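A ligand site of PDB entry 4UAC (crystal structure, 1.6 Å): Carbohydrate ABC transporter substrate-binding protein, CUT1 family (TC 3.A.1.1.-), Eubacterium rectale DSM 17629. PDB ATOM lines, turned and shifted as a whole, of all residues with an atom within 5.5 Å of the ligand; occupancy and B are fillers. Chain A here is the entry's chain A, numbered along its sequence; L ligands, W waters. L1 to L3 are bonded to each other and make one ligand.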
ATOM      1  N   PRO A  27     -23.856  -9.348  -1.875  1.00  0.00           N
ATOM      2  CA  PRO A  27     -24.379  -8.115  -1.277  1.00  0.00           C
ATOM      3  C   PRO A  27     -25.106  -7.226  -2.275  1.00  0.00           C
ATOM      4  O   PRO A  27     -24.906  -7.347  -3.478  1.00  0.00           O
ATOM      5  CB  PRO A  27     -23.133  -7.422  -0.737  1.00  0.00           C
ATOM      6  CG  PRO A  27     -21.991  -7.958  -1.605  1.00  0.00           C
ATOM      7  CD  PRO A  27     -22.378  -9.378  -1.923  1.00  0.00           C
ATOM      8  N   GLU A  29     -24.823  -4.254  -3.250  1.00  0.00           N
ATOM      9  CA  GLU A  29     -23.996  -3.465  -4.144  1.00  0.00           C
ATOM     10  C   GLU A  29     -23.552  -4.250  -5.380  1.00  0.00           C
ATOM     11  O   GLU A  29     -23.345  -3.673  -6.430  1.00  0.00           O
ATOM     12  CB  GLU A  29     -22.757  -2.936  -3.400  1.00  0.00           C
ATOM     13  CG  GLU A  29     -23.080  -1.956  -2.256  1.00  0.00           C
ATOM     14  CD  GLU A  29     -23.409  -2.602  -0.914  1.00  0.00           C
ATOM     15  OE1 GLU A  29     -23.453  -3.852  -0.788  1.00  0.00           O
ATOM     16  OE2 GLU A  29     -23.634  -1.832   0.039  1.00  0.00           O
ATOM     17  N   SER A  63     -25.430  -9.313   2.794  1.00  0.00           N
ATOM     18  CA  SER A  63     -24.061  -8.915   3.095  1.00  0.00           C
ATOM     19  C   SER A  63     -23.204 -10.129   3.403  1.00  0.00           C
ATOM     20  O   SER A  63     -23.644 -11.055   4.069  1.00  0.00           O
ATOM     21  CB  SER A  63     -24.059  -7.975   4.303  1.00  0.00           C
ATOM     22  OG  SER A  63     -22.726  -7.691   4.704  1.00  0.00           O
ATOM     23  N   GLU A  64     -21.956 -10.087   2.970  1.00  0.00           N
ATOM     24  CA  GLU A  64     -21.004 -11.119   3.386  1.00  0.00           C
ATOM     25  C   GLU A  64     -20.882 -11.257   4.914  1.00  0.00           C
ATOM     26  O   GLU A  64     -20.543 -12.336   5.419  1.00  0.00           O
ATOM     27  CB  GLU A  64     -19.617 -10.831   2.797  1.00  0.00           C
ATOM     28  CG  GLU A  64     -19.575 -10.794   1.276  1.00  0.00           C
ATOM     29  CD  GLU A  64     -19.606  -9.363   0.731  1.00  0.00           C
ATOM     30  OE1 GLU A  64     -20.369  -8.532   1.257  1.00  0.00           O
ATOM     31  OE2 GLU A  64     -18.839  -9.050  -0.211  1.00  0.00           O
ATOM     32  N   SER A  65     -21.136 -10.168   5.641  1.00  0.00           N
ATOM     33  CA  SER A  65     -21.039 -10.180   7.092  1.00  0.00           C
ATOM     34  C   SER A  65     -22.120 -11.029   7.746  1.00  0.00           C
ATOM     35  O   SER A  65     -21.948 -11.492   8.858  1.00  0.00           O
ATOM     36  CB  SER A  65     -21.113  -8.737   7.637  1.00  0.00           C
ATOM     37  OG  SER A  65     -22.418  -8.212   7.502  1.00  0.00           O
ATOM     38  N   LYS A  68     -22.934 -16.299   7.321  1.00  0.00           N
ATOM     39  CA  LYS A  68     -22.956 -17.394   8.276  1.00  0.00           C
ATOM     40  C   LYS A  68     -24.367 -17.574   8.833  1.00  0.00           C
ATOM     41  O   LYS A  68     -24.893 -18.691   8.860  1.00  0.00           O
ATOM     42  CB  LYS A  68     -21.972 -17.185   9.431  1.00  0.00           C
ATOM     43  CG  LYS A  68     -22.173 -18.190  10.587  1.00  0.00           C
ATOM     44  CD  LYS A  68     -21.216 -17.962  11.734  1.00  0.00           C
ATOM     45  CE  LYS A  68     -21.714 -16.877  12.622  1.00  0.00           C
ATOM     46  NZ  LYS A  68     -22.923 -17.299  13.378  1.00  0.00           N
ATOM     47  N   ASP A  69     -24.960 -16.483   9.288  1.00  0.00           N
ATOM     48  CA  ASP A  69     -26.290 -16.538   9.902  1.00  0.00           C
ATOM     49  C   ASP A  69     -27.330 -17.068   8.908  1.00  0.00           C
ATOM     50  O   ASP A  69     -28.157 -17.936   9.225  1.00  0.00           O
ATOM     51  CB  ASP A  69     -26.703 -15.152  10.396  1.00  0.00           C
ATOM     52  CG  ASP A  69     -25.920 -14.707  11.602  1.00  0.00           C
ATOM     53  OD1 ASP A  69     -25.390 -15.577  12.330  1.00  0.00           O
ATOM     54  OD2 ASP A  69     -25.866 -13.491  11.855  1.00  0.00           O
ATOM     55  N   ALA A  85     -17.537 -13.831   4.457  1.00  0.00           N
ATOM     56  CA  ALA A  85     -16.292 -13.387   5.092  1.00  0.00           C
ATOM     57  C   ALA A  85     -15.607 -14.563   5.756  1.00  0.00           C
ATOM     58  O   ALA A  85     -16.236 -15.364   6.429  1.00  0.00           O
ATOM     59  CB  ALA A  85     -16.561 -12.299   6.108  1.00  0.00           C
ATOM     60  N   ASP A  87     -13.876 -15.474   8.290  1.00  0.00           N
ATOM     61  CA  ASP A  87     -13.954 -15.836   9.703  1.00  0.00           C
ATOM     62  C   ASP A  87     -15.148 -16.741   9.961  1.00  0.00           C
ATOM     63  O   ASP A  87     -15.254 -17.372  11.030  1.00  0.00           O
ATOM     64  CB  ASP A  87     -14.058 -14.597  10.566  1.00  0.00           C
ATOM     65  CG  ASP A  87     -15.252 -13.765  10.196  1.00  0.00           C
ATOM     66  OD1 ASP A  87     -15.167 -13.013   9.198  1.00  0.00           O
ATOM     67  OD2 ASP A  87     -16.310 -13.915  10.847  1.00  0.00           O
ATOM     68  N   GLN A  88     -16.051 -16.783   8.999  1.00  0.00           N
ATOM     69  CA  GLN A  88     -17.237 -17.655   9.102  1.00  0.00           C
ATOM     70  C   GLN A  88     -16.980 -19.095   8.718  1.00  0.00           C
ATOM     71  O   GLN A  88     -17.868 -19.950   8.815  1.00  0.00           O
ATOM     72  CB  GLN A  88     -18.341 -17.080   8.231  1.00  0.00           C
ATOM     73  CG  GLN A  88     -18.836 -15.708   8.719  1.00  0.00           C
ATOM     74  CD  GLN A  88     -19.513 -14.905   7.633  1.00  0.00           C
ATOM     75  OE1 GLN A  88     -19.786 -15.407   6.567  1.00  0.00           O
ATOM     76  NE2 GLN A  88     -19.744 -13.638   7.892  1.00  0.00           N
ATOM     77  N   ASN A 135      -9.894  -8.712   3.088  1.00  0.00           N
ATOM     78  CA  ASN A 135     -10.923  -8.216   4.000  1.00  0.00           C
ATOM     79  C   ASN A 135     -10.268  -7.601   5.214  1.00  0.00           C
ATOM     80  O   ASN A 135      -9.728  -8.305   6.076  1.00  0.00           O
ATOM     81  CB  ASN A 135     -11.854  -9.343   4.414  1.00  0.00           C
ATOM     82  CG  ASN A 135     -13.154  -8.820   5.001  1.00  0.00           C
ATOM     83  OD1 ASN A 135     -13.669  -7.785   4.571  1.00  0.00           O
ATOM     84  ND2 ASN A 135     -13.689  -9.550   5.972  1.00  0.00           N
ATOM     85  N   ASN A 169     -18.468  -2.807  17.523  1.00  0.00           N
ATOM     86  CA  ASN A 169     -18.255  -3.819  16.485  1.00  0.00           C
ATOM     87  C   ASN A 169     -16.944  -4.534  16.735  1.00  0.00           C
ATOM     88  O   ASN A 169     -15.872  -3.919  16.666  1.00  0.00           O
ATOM     89  CB  ASN A 169     -18.298  -3.134  15.112  1.00  0.00           C
ATOM     90  CG  ASN A 169     -18.249  -4.111  13.964  1.00  0.00           C
ATOM     91  OD1 ASN A 169     -17.548  -5.131  14.023  1.00  0.00           O
ATOM     92  ND2 ASN A 169     -19.008  -3.809  12.904  1.00  0.00           N
ATOM     93  N   GLY A 170     -17.005  -5.809  17.097  1.00  0.00           N
ATOM     94  CA  GLY A 170     -15.807  -6.532  17.473  1.00  0.00           C
ATOM     95  C   GLY A 170     -14.738  -6.611  16.396  1.00  0.00           C
ATOM     96  O   GLY A 170     -13.553  -6.779  16.703  1.00  0.00           O
ATOM     97  N   TRP A 171     -15.153  -6.501  15.142  1.00  0.00           N
ATOM     98  CA  TRP A 171     -14.207  -6.569  14.035  1.00  0.00           C
ATOM     99  C   TRP A 171     -13.261  -5.366  14.028  1.00  0.00           C
ATOM    100  O   TRP A 171     -12.157  -5.447  13.478  1.00  0.00           O
ATOM    101  CB  TRP A 171     -14.971  -6.687  12.713  1.00  0.00           C
ATOM    102  CG  TRP A 171     -14.170  -7.084  11.536  1.00  0.00           C
ATOM    103  CD1 TRP A 171     -13.458  -8.248  11.363  1.00  0.00           C
ATOM    104  CD2 TRP A 171     -13.992  -6.330  10.338  1.00  0.00           C
ATOM    105  NE1 TRP A 171     -12.853  -8.262  10.124  1.00  0.00           N
ATOM    106  CE2 TRP A 171     -13.167  -7.094   9.471  1.00  0.00           C
ATOM    107  CE3 TRP A 171     -14.459  -5.092   9.893  1.00  0.00           C
ATOM    108  CZ2 TRP A 171     -12.818  -6.632   8.210  1.00  0.00           C
ATOM    109  CZ3 TRP A 171     -14.113  -4.654   8.635  1.00  0.00           C
ATOM    110  CH2 TRP A 171     -13.303  -5.415   7.805  1.00  0.00           C
ATOM    111  N   TYR A 172     -13.694  -4.280  14.680  1.00  0.00           N
ATOM    112  CA  TYR A 172     -12.923  -3.048  14.861  1.00  0.00           C
ATOM    113  C   TYR A 172     -12.300  -2.903  16.263  1.00  0.00           C
ATOM    114  O   TYR A 172     -11.188  -2.382  16.413  1.00  0.00           O
ATOM    115  CB  TYR A 172     -13.804  -1.848  14.576  1.00  0.00           C
ATOM    116  CG  TYR A 172     -14.291  -1.728  13.158  1.00  0.00           C
ATOM    117  CD1 TYR A 172     -13.570  -0.999  12.226  1.00  0.00           C
ATOM    118  CD2 TYR A 172     -15.467  -2.322  12.757  1.00  0.00           C
ATOM    119  CE1 TYR A 172     -14.009  -0.872  10.918  1.00  0.00           C
ATOM    120  CE2 TYR A 172     -15.909  -2.218  11.453  1.00  0.00           C
ATOM    121  CZ  TYR A 172     -15.195  -1.490  10.544  1.00  0.00           C
ATOM    122  OH  TYR A 172     -15.654  -1.389   9.265  1.00  0.00           O
ATOM    123  N   ASN A 223     -22.623   0.516  14.739  1.00  0.00           N
ATOM    124  CA  ASN A 223     -22.074  -0.791  14.436  1.00  0.00           C
ATOM    125  C   ASN A 223     -21.699  -0.979  12.976  1.00  0.00           C
ATOM    126  O   ASN A 223     -20.596  -1.494  12.674  1.00  0.00           O
ATOM    127  CB  ASN A 223     -23.079  -1.863  14.868  1.00  0.00           C
ATOM    128  CG  ASN A 223     -22.512  -3.257  14.782  1.00  0.00           C
ATOM    129  OD1 ASN A 223     -22.723  -3.951  13.784  1.00  0.00           O
ATOM    130  ND2 ASN A 223     -21.749  -3.646  15.788  1.00  0.00           N
ATOM    131  N   GLU A 224     -22.551  -0.562  12.047  1.00  0.00           N
ATOM    132  CA  GLU A 224     -22.212  -0.779  10.640  1.00  0.00           C
ATOM    133  C   GLU A 224     -21.872   0.498   9.876  1.00  0.00           C
ATOM    134  O   GLU A 224     -21.794   0.505   8.652  1.00  0.00           O
ATOM    135  CB  GLU A 224     -23.321  -1.592   9.977  1.00  0.00           C
ATOM    136  CG  GLU A 224     -23.158  -3.079  10.346  1.00  0.00           C
ATOM    137  CD  GLU A 224     -24.169  -3.976   9.693  1.00  0.00           C
ATOM    138  OE1 GLU A 224     -25.320  -3.535   9.465  1.00  0.00           O
ATOM    139  OE2 GLU A 224     -23.817  -5.149   9.425  1.00  0.00           O
ATOM    140  N   TRP A 245     -15.910  -1.405   0.666  1.00  0.00           N
ATOM    141  CA  TRP A 245     -17.293  -1.461   0.198  1.00  0.00           C
ATOM    142  C   TRP A 245     -17.997  -0.101   0.221  1.00  0.00           C
ATOM    143  O   TRP A 245     -18.993   0.087  -0.491  1.00  0.00           O
ATOM    144  CB  TRP A 245     -18.088  -2.482   1.032  1.00  0.00           C
ATOM    145  CG  TRP A 245     -17.999  -2.195   2.473  1.00  0.00           C
ATOM    146  CD1 TRP A 245     -18.845  -1.406   3.191  1.00  0.00           C
ATOM    147  CD2 TRP A 245     -16.994  -2.644   3.393  1.00  0.00           C
ATOM    148  NE1 TRP A 245     -18.431  -1.326   4.492  1.00  0.00           N
ATOM    149  CE2 TRP A 245     -17.287  -2.073   4.632  1.00  0.00           C
ATOM    150  CE3 TRP A 245     -15.864  -3.460   3.271  1.00  0.00           C
ATOM    151  CZ2 TRP A 245     -16.505  -2.299   5.759  1.00  0.00           C
ATOM    152  CZ3 TRP A 245     -15.087  -3.674   4.392  1.00  0.00           C
ATOM    153  CH2 TRP A 245     -15.405  -3.092   5.619  1.00  0.00           C
ATOM    154  N   LYS A 283     -12.725 -11.997   1.779  1.00  0.00           N
ATOM    155  CA  LYS A 283     -14.074 -12.409   1.391  1.00  0.00           C
ATOM    156  C   LYS A 283     -13.934 -13.376   0.235  1.00  0.00           C
ATOM    157  O   LYS A 283     -13.090 -13.195  -0.645  1.00  0.00           O
ATOM    158  CB  LYS A 283     -14.924 -11.201   1.046  1.00  0.00           C
ATOM    159  CG  LYS A 283     -15.033 -10.246   2.245  1.00  0.00           C
ATOM    160  CD  LYS A 283     -16.129  -9.154   2.065  1.00  0.00           C
ATOM    161  CE  LYS A 283     -15.749  -8.145   0.984  1.00  0.00           C
ATOM    162  NZ  LYS A 283     -16.812  -7.126   0.758  1.00  0.00           N
ATOM    163  N   ARG A 317     -16.919  -1.270  -9.391  1.00  0.00           N
ATOM    164  CA  ARG A 317     -17.188  -0.579  -8.136  1.00  0.00           C
ATOM    165  C   ARG A 317     -15.987  -0.456  -7.201  1.00  0.00           C
ATOM    166  O   ARG A 317     -16.142  -0.257  -5.981  1.00  0.00           O
ATOM    167  CB  ARG A 317     -18.393  -1.251  -7.440  1.00  0.00           C
ATOM    168  CG  ARG A 317     -18.309  -2.739  -7.237  1.00  0.00           C
ATOM    169  CD  ARG A 317     -19.472  -3.244  -6.337  1.00  0.00           C
ATOM    170  NE  ARG A 317     -19.374  -2.659  -4.998  1.00  0.00           N
ATOM    171  CZ  ARG A 317     -19.425  -3.325  -3.846  1.00  0.00           C
ATOM    172  NH1 ARG A 317     -19.587  -4.639  -3.834  1.00  0.00           N
ATOM    173  NH2 ARG A 317     -19.309  -2.656  -2.701  1.00  0.00           N
ATOM    174  N   TRP A 361     -17.310 -12.120  19.152  1.00  0.00           N
ATOM    175  CA  TRP A 361     -18.177 -11.214  18.417  1.00  0.00           C
ATOM    176  C   TRP A 361     -19.378 -10.816  19.272  1.00  0.00           C
ATOM    177  O   TRP A 361     -19.813  -9.663  19.258  1.00  0.00           O
ATOM    178  CB  TRP A 361     -18.697 -11.835  17.121  1.00  0.00           C
ATOM    179  CG  TRP A 361     -17.701 -12.395  16.162  1.00  0.00           C
ATOM    180  CD1 TRP A 361     -17.687 -13.660  15.664  1.00  0.00           C
ATOM    181  CD2 TRP A 361     -16.598 -11.717  15.560  1.00  0.00           C
ATOM    182  NE1 TRP A 361     -16.644 -13.829  14.792  1.00  0.00           N
ATOM    183  CE2 TRP A 361     -15.958 -12.643  14.704  1.00  0.00           C
ATOM    184  CE3 TRP A 361     -16.081 -10.417  15.646  1.00  0.00           C
ATOM    185  CZ2 TRP A 361     -14.830 -12.314  13.946  1.00  0.00           C
ATOM    186  CZ3 TRP A 361     -14.946 -10.104  14.903  1.00  0.00           C
ATOM    187  CH2 TRP A 361     -14.330 -11.045  14.070  1.00  0.00           C
ATOM    188  N   ASP A 362     -19.900 -11.773  20.025  1.00  0.00           N
ATOM    189  CA  ASP A 362     -21.071 -11.530  20.870  1.00  0.00           C
ATOM    190  C   ASP A 362     -20.755 -10.613  22.043  1.00  0.00           C
ATOM    191  O   ASP A 362     -21.507  -9.678  22.296  1.00  0.00           O
ATOM    192  CB  ASP A 362     -21.630 -12.849  21.392  1.00  0.00           C
ATOM    193  CG  ASP A 362     -22.379 -13.651  20.320  1.00  0.00           C
ATOM    194  OD1 ASP A 362     -22.597 -13.138  19.194  1.00  0.00           O
ATOM    195  OD2 ASP A 362     -22.754 -14.809  20.622  1.00  0.00           O
ATOM    196  N   THR A 365     -19.908  -6.413  21.509  1.00  0.00           N
ATOM    197  CA  THR A 365     -20.877  -5.375  21.254  1.00  0.00           C
ATOM    198  C   THR A 365     -21.375  -4.704  22.551  1.00  0.00           C
ATOM    199  O   THR A 365     -21.293  -3.475  22.681  1.00  0.00           O
ATOM    200  CB  THR A 365     -22.032  -5.926  20.414  1.00  0.00           C
ATOM    201  OG1 THR A 365     -21.510  -6.388  19.155  1.00  0.00           O
ATOM    202  CG2 THR A 365     -23.072  -4.851  20.169  1.00  0.00           C
HETATM  203  C1  LIG L   1     -21.170  -4.846   2.734  1.00  0.00           C
HETATM  204  C2  LIG L   1     -19.763  -5.314   2.435  1.00  0.00           C
HETATM  205  C3  LIG L   1     -19.196  -6.132   3.533  1.00  0.00           C
HETATM  206  C4  LIG L   1     -19.192  -5.381   4.826  1.00  0.00           C
HETATM  207  C5  LIG L   1     -20.606  -4.941   5.160  1.00  0.00           C
HETATM  208  C6  LIG L   1     -20.646  -3.998   6.314  1.00  0.00           C
HETATM  209  O1  LIG L   1     -22.047  -5.913   2.739  1.00  0.00           O
HETATM  210  O2  LIG L   1     -19.713  -5.989   1.145  1.00  0.00           O
HETATM  211  O3  LIG L   1     -17.816  -6.453   3.186  1.00  0.00           O
HETATM  212  O4  LIG L   1     -18.666  -6.197   5.870  1.00  0.00           O
HETATM  213  O5  LIG L   1     -21.182  -4.176   4.055  1.00  0.00           O
HETATM  214  O6  LIG L   1     -22.010  -3.686   6.611  1.00  0.00           O
HETATM  215  C1  LG2 L   2     -17.483  -5.724   6.433  1.00  0.00           C
HETATM  216  C2  LG2 L   2     -16.506  -6.855   6.466  1.00  0.00           C
HETATM  217  C3  LG2 L   2     -16.996  -7.981   7.325  1.00  0.00           C
HETATM  218  C4  LG2 L   2     -17.289  -7.515   8.711  1.00  0.00           C
HETATM  219  C5  LG2 L   2     -18.220  -6.315   8.692  1.00  0.00           C
HETATM  220  C6  LG2 L   2     -18.346  -5.728  10.079  1.00  0.00           C
HETATM  221  O1  LG2 L   2     -16.284  -7.306   5.115  1.00  0.00           O
HETATM  222  O2  LG2 L   2     -16.008  -9.040   7.348  1.00  0.00           O
HETATM  223  O3  LG2 L   2     -17.901  -8.582   9.503  1.00  0.00           O
HETATM  224  O4  LG2 L   2     -17.722  -5.267   7.814  1.00  0.00           O
HETATM  225  O5  LG2 L   2     -19.294  -4.642  10.088  1.00  0.00           O
HETATM  226  C1  LG3 L   3     -17.048  -9.204  10.422  1.00  0.00           C
HETATM  227  O1  LG3 L   3     -16.817 -11.066   8.949  1.00  0.00           O
HETATM  228  C2  LG3 L   3     -17.173 -10.699  10.305  1.00  0.00           C
HETATM  229  C3  LG3 L   3     -23.117 -12.545  14.668  1.00  0.00           C
HETATM  230  C4  LG3 L   3     -18.549 -11.157  10.620  1.00  0.00           C
HETATM  231  O2  LG3 L   3     -18.670 -12.586  10.504  1.00  0.00           O
HETATM  232  C5  LG3 L   3     -18.889 -10.741  12.023  1.00  0.00           C
HETATM  233  N1  LG3 L   3     -20.221 -11.263  12.380  1.00  0.00           N
HETATM  234  C6  LG3 L   3     -18.815  -9.239  12.102  1.00  0.00           C
HETATM  235  O3  LG3 L   3     -17.456  -8.795  11.786  1.00  0.00           O
HETATM  236  C7  LG3 L   3     -19.044  -8.668  13.477  1.00  0.00           C
HETATM  237  C8  LG3 L   3     -20.280 -11.961  13.687  1.00  0.00           C
HETATM  238  C9  LG3 L   3     -21.119 -13.356  13.464  1.00  0.00           C
HETATM  239  O4  LG3 L   3     -20.566 -13.962  12.221  1.00  0.00           O
HETATM  240  C10 LG3 L   3     -22.397 -13.125  13.336  1.00  0.00           C
HETATM  241  O5  LG3 L   3     -23.133 -14.409  13.028  1.00  0.00           O
HETATM  242  O6  LG3 L   3     -24.490 -12.214  14.437  1.00  0.00           O
HETATM  243  C11 LG3 L   3     -22.420 -11.400  15.210  1.00  0.00           C
HETATM  244  C12 LG3 L   3     -20.846 -11.117  14.669  1.00  0.00           C
HETATM  245  C13 LG3 L   3     -23.023 -10.475  16.221  1.00  0.00           C
HETATM  246  O7  LG3 L   3     -21.996 -10.130  17.096  1.00  0.00           O
HETATM  247  O   HOH W   1     -18.298 -15.577  12.177  1.00  0.00           O
HETATM  248  O   HOH W   2     -22.701  -1.393   2.838  1.00  0.00           O
HETATM  249  O   HOH W   3     -23.876  -5.881   7.003  1.00  0.00           O
HETATM  250  O   HOH W   4     -24.289  -4.820   1.721  1.00  0.00           O
HETATM  251  O   HOH W   5     -22.963  -1.452   5.341  1.00  0.00           O
HETATM  252  O   HOH W   6     -22.941 -14.053   9.753  1.00  0.00           O
HETATM  253  O   HOH W   7     -18.331  -2.162   9.007  1.00  0.00           O
HETATM  254  O   HOH W   8     -22.424  -9.804  11.298  1.00  0.00           O
HETATM  255  O   HOH W   9     -21.642  -6.275  10.307  1.00  0.00           O
HETATM  256  O   HOH W  10     -20.659  -4.524  -0.945  1.00  0.00           O
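O of Glu 64 lies within hydrogen-bond range of NE2 of Gln 88.
The side-chain amide oxygen of Gln 88 lies within hydrogen-bond range of the backbone NH of Ala 85, at 3.5 Å.
ND2 of Asn 169 sits at hydrogen-bond distance from O of Asn 223 (2.8 Å).
O of Glu 64 lies within hydrogen-bond range of N of Ala 85, 3.5 Å away.
OG of Ser 63 lies within hydrogen-bond range of OG of Ser 65, at 2.9 Å.
OD1 of Asn 169 is in hydrogen-bond range of N of Trp 171, at 3.0 Å.
N of Lys 68 lies within hydrogen-bond range of OE1 of Gln 88, 3.4 Å away.
OE2 of Glu 64 is in salt-bridge range of NZ of Lys 283.
An oxygen (O1) of LIG L1 lies within hydrogen-bond range of the side-chain hydroxyl (OG) of Ser 63, 2.7 Å away.
An oxygen (O3) of LIG L1 lies within hydrogen-bond range of the side-chain amino group (NZ) of Lys 283, at 2.7 Å.
An oxygen (O2) of LIG L1 sits at hydrogen-bond distance from the side-chain carboxylate (OE1) of Glu 64 (2.6 Å).
The side-chain amide nitrogen (NE2) of Gln 88 sits at hydrogen-bond distance from an oxygen (O2) of LG3 L3 (3.0 Å).
The side-chain carboxylate (OD1) of Asp 87 sits at hydrogen-bond distance from an oxygen (O1) of LG3 L3.
O7 of LG3 L3 sits at hydrogen-bond distance from O of Trp 361, at 3.1 Å.
The side-chain amide nitrogen (ND2) of Asn 169 is in hydrogen-bond range of an oxygen (O5) of LG2 L2 (3.0 Å).
OD1 of Asn 135 lies within hydrogen-bond range of O1 of LG2 L2.
OD1 of Asp 69 lies within hydrogen-bond range of O5 of LG3 L3 (2.6 Å).
The side-chain amino group (NZ) of Lys 68 lies close to an oxygen (O5) of LG3 L3.
Water W4 lies within hydrogen-bond range of an oxygen (O1) of LIG L1 (2.7 Å) and the side-chain carboxylate (OE1) of Glu 29 (2.8 Å).
Water W10 lies within hydrogen-bond range of an oxygen (O2) of LIG L1 (2.7 Å), the side-chain carboxylate of Glu 29 (2.9 Å) and the guanidinium group of Arg 317 (2.9 Å).
Water W1 bridges an oxygen (O4) of LG3 L3 (2.8 Å) and the side-chain carboxylate of Asp 87 (2.9 Å).
Water W9 lies within hydrogen-bond range of OE2 of Glu 224 (2.6 Å), O5 of LG2 L2 (2.9 Å) and OG of Ser 65 (3.5 Å).
Water W3 lies within hydrogen-bond range of OE2 of Glu 224 (2.5 Å), OG of Ser 65 (2.8 Å), O6 of LIG L1 (2.9 Å) and OG of Ser 63 (3.1 Å).
Water W6 lies within hydrogen-bond range of O of Ser 65 (2.9 Å), N of Asp 69 (3.2 Å), O5 of LG3 L3 (3.3 Å) and N of Lys 68 (3.3 Å).
Residues that only touch the ligand: Pro 27 (3.9 Å), Ser 65 (3.7 Å), Ala 85 (3.1 Å), Trp 171 (3.4 Å), Glu 224 (3.7 Å), Trp 245 (3.5 Å) and Asp 362 (3.7 Å).
The nearest printed residue that does not touch the ligand is Asn 223 (4.3 Å).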
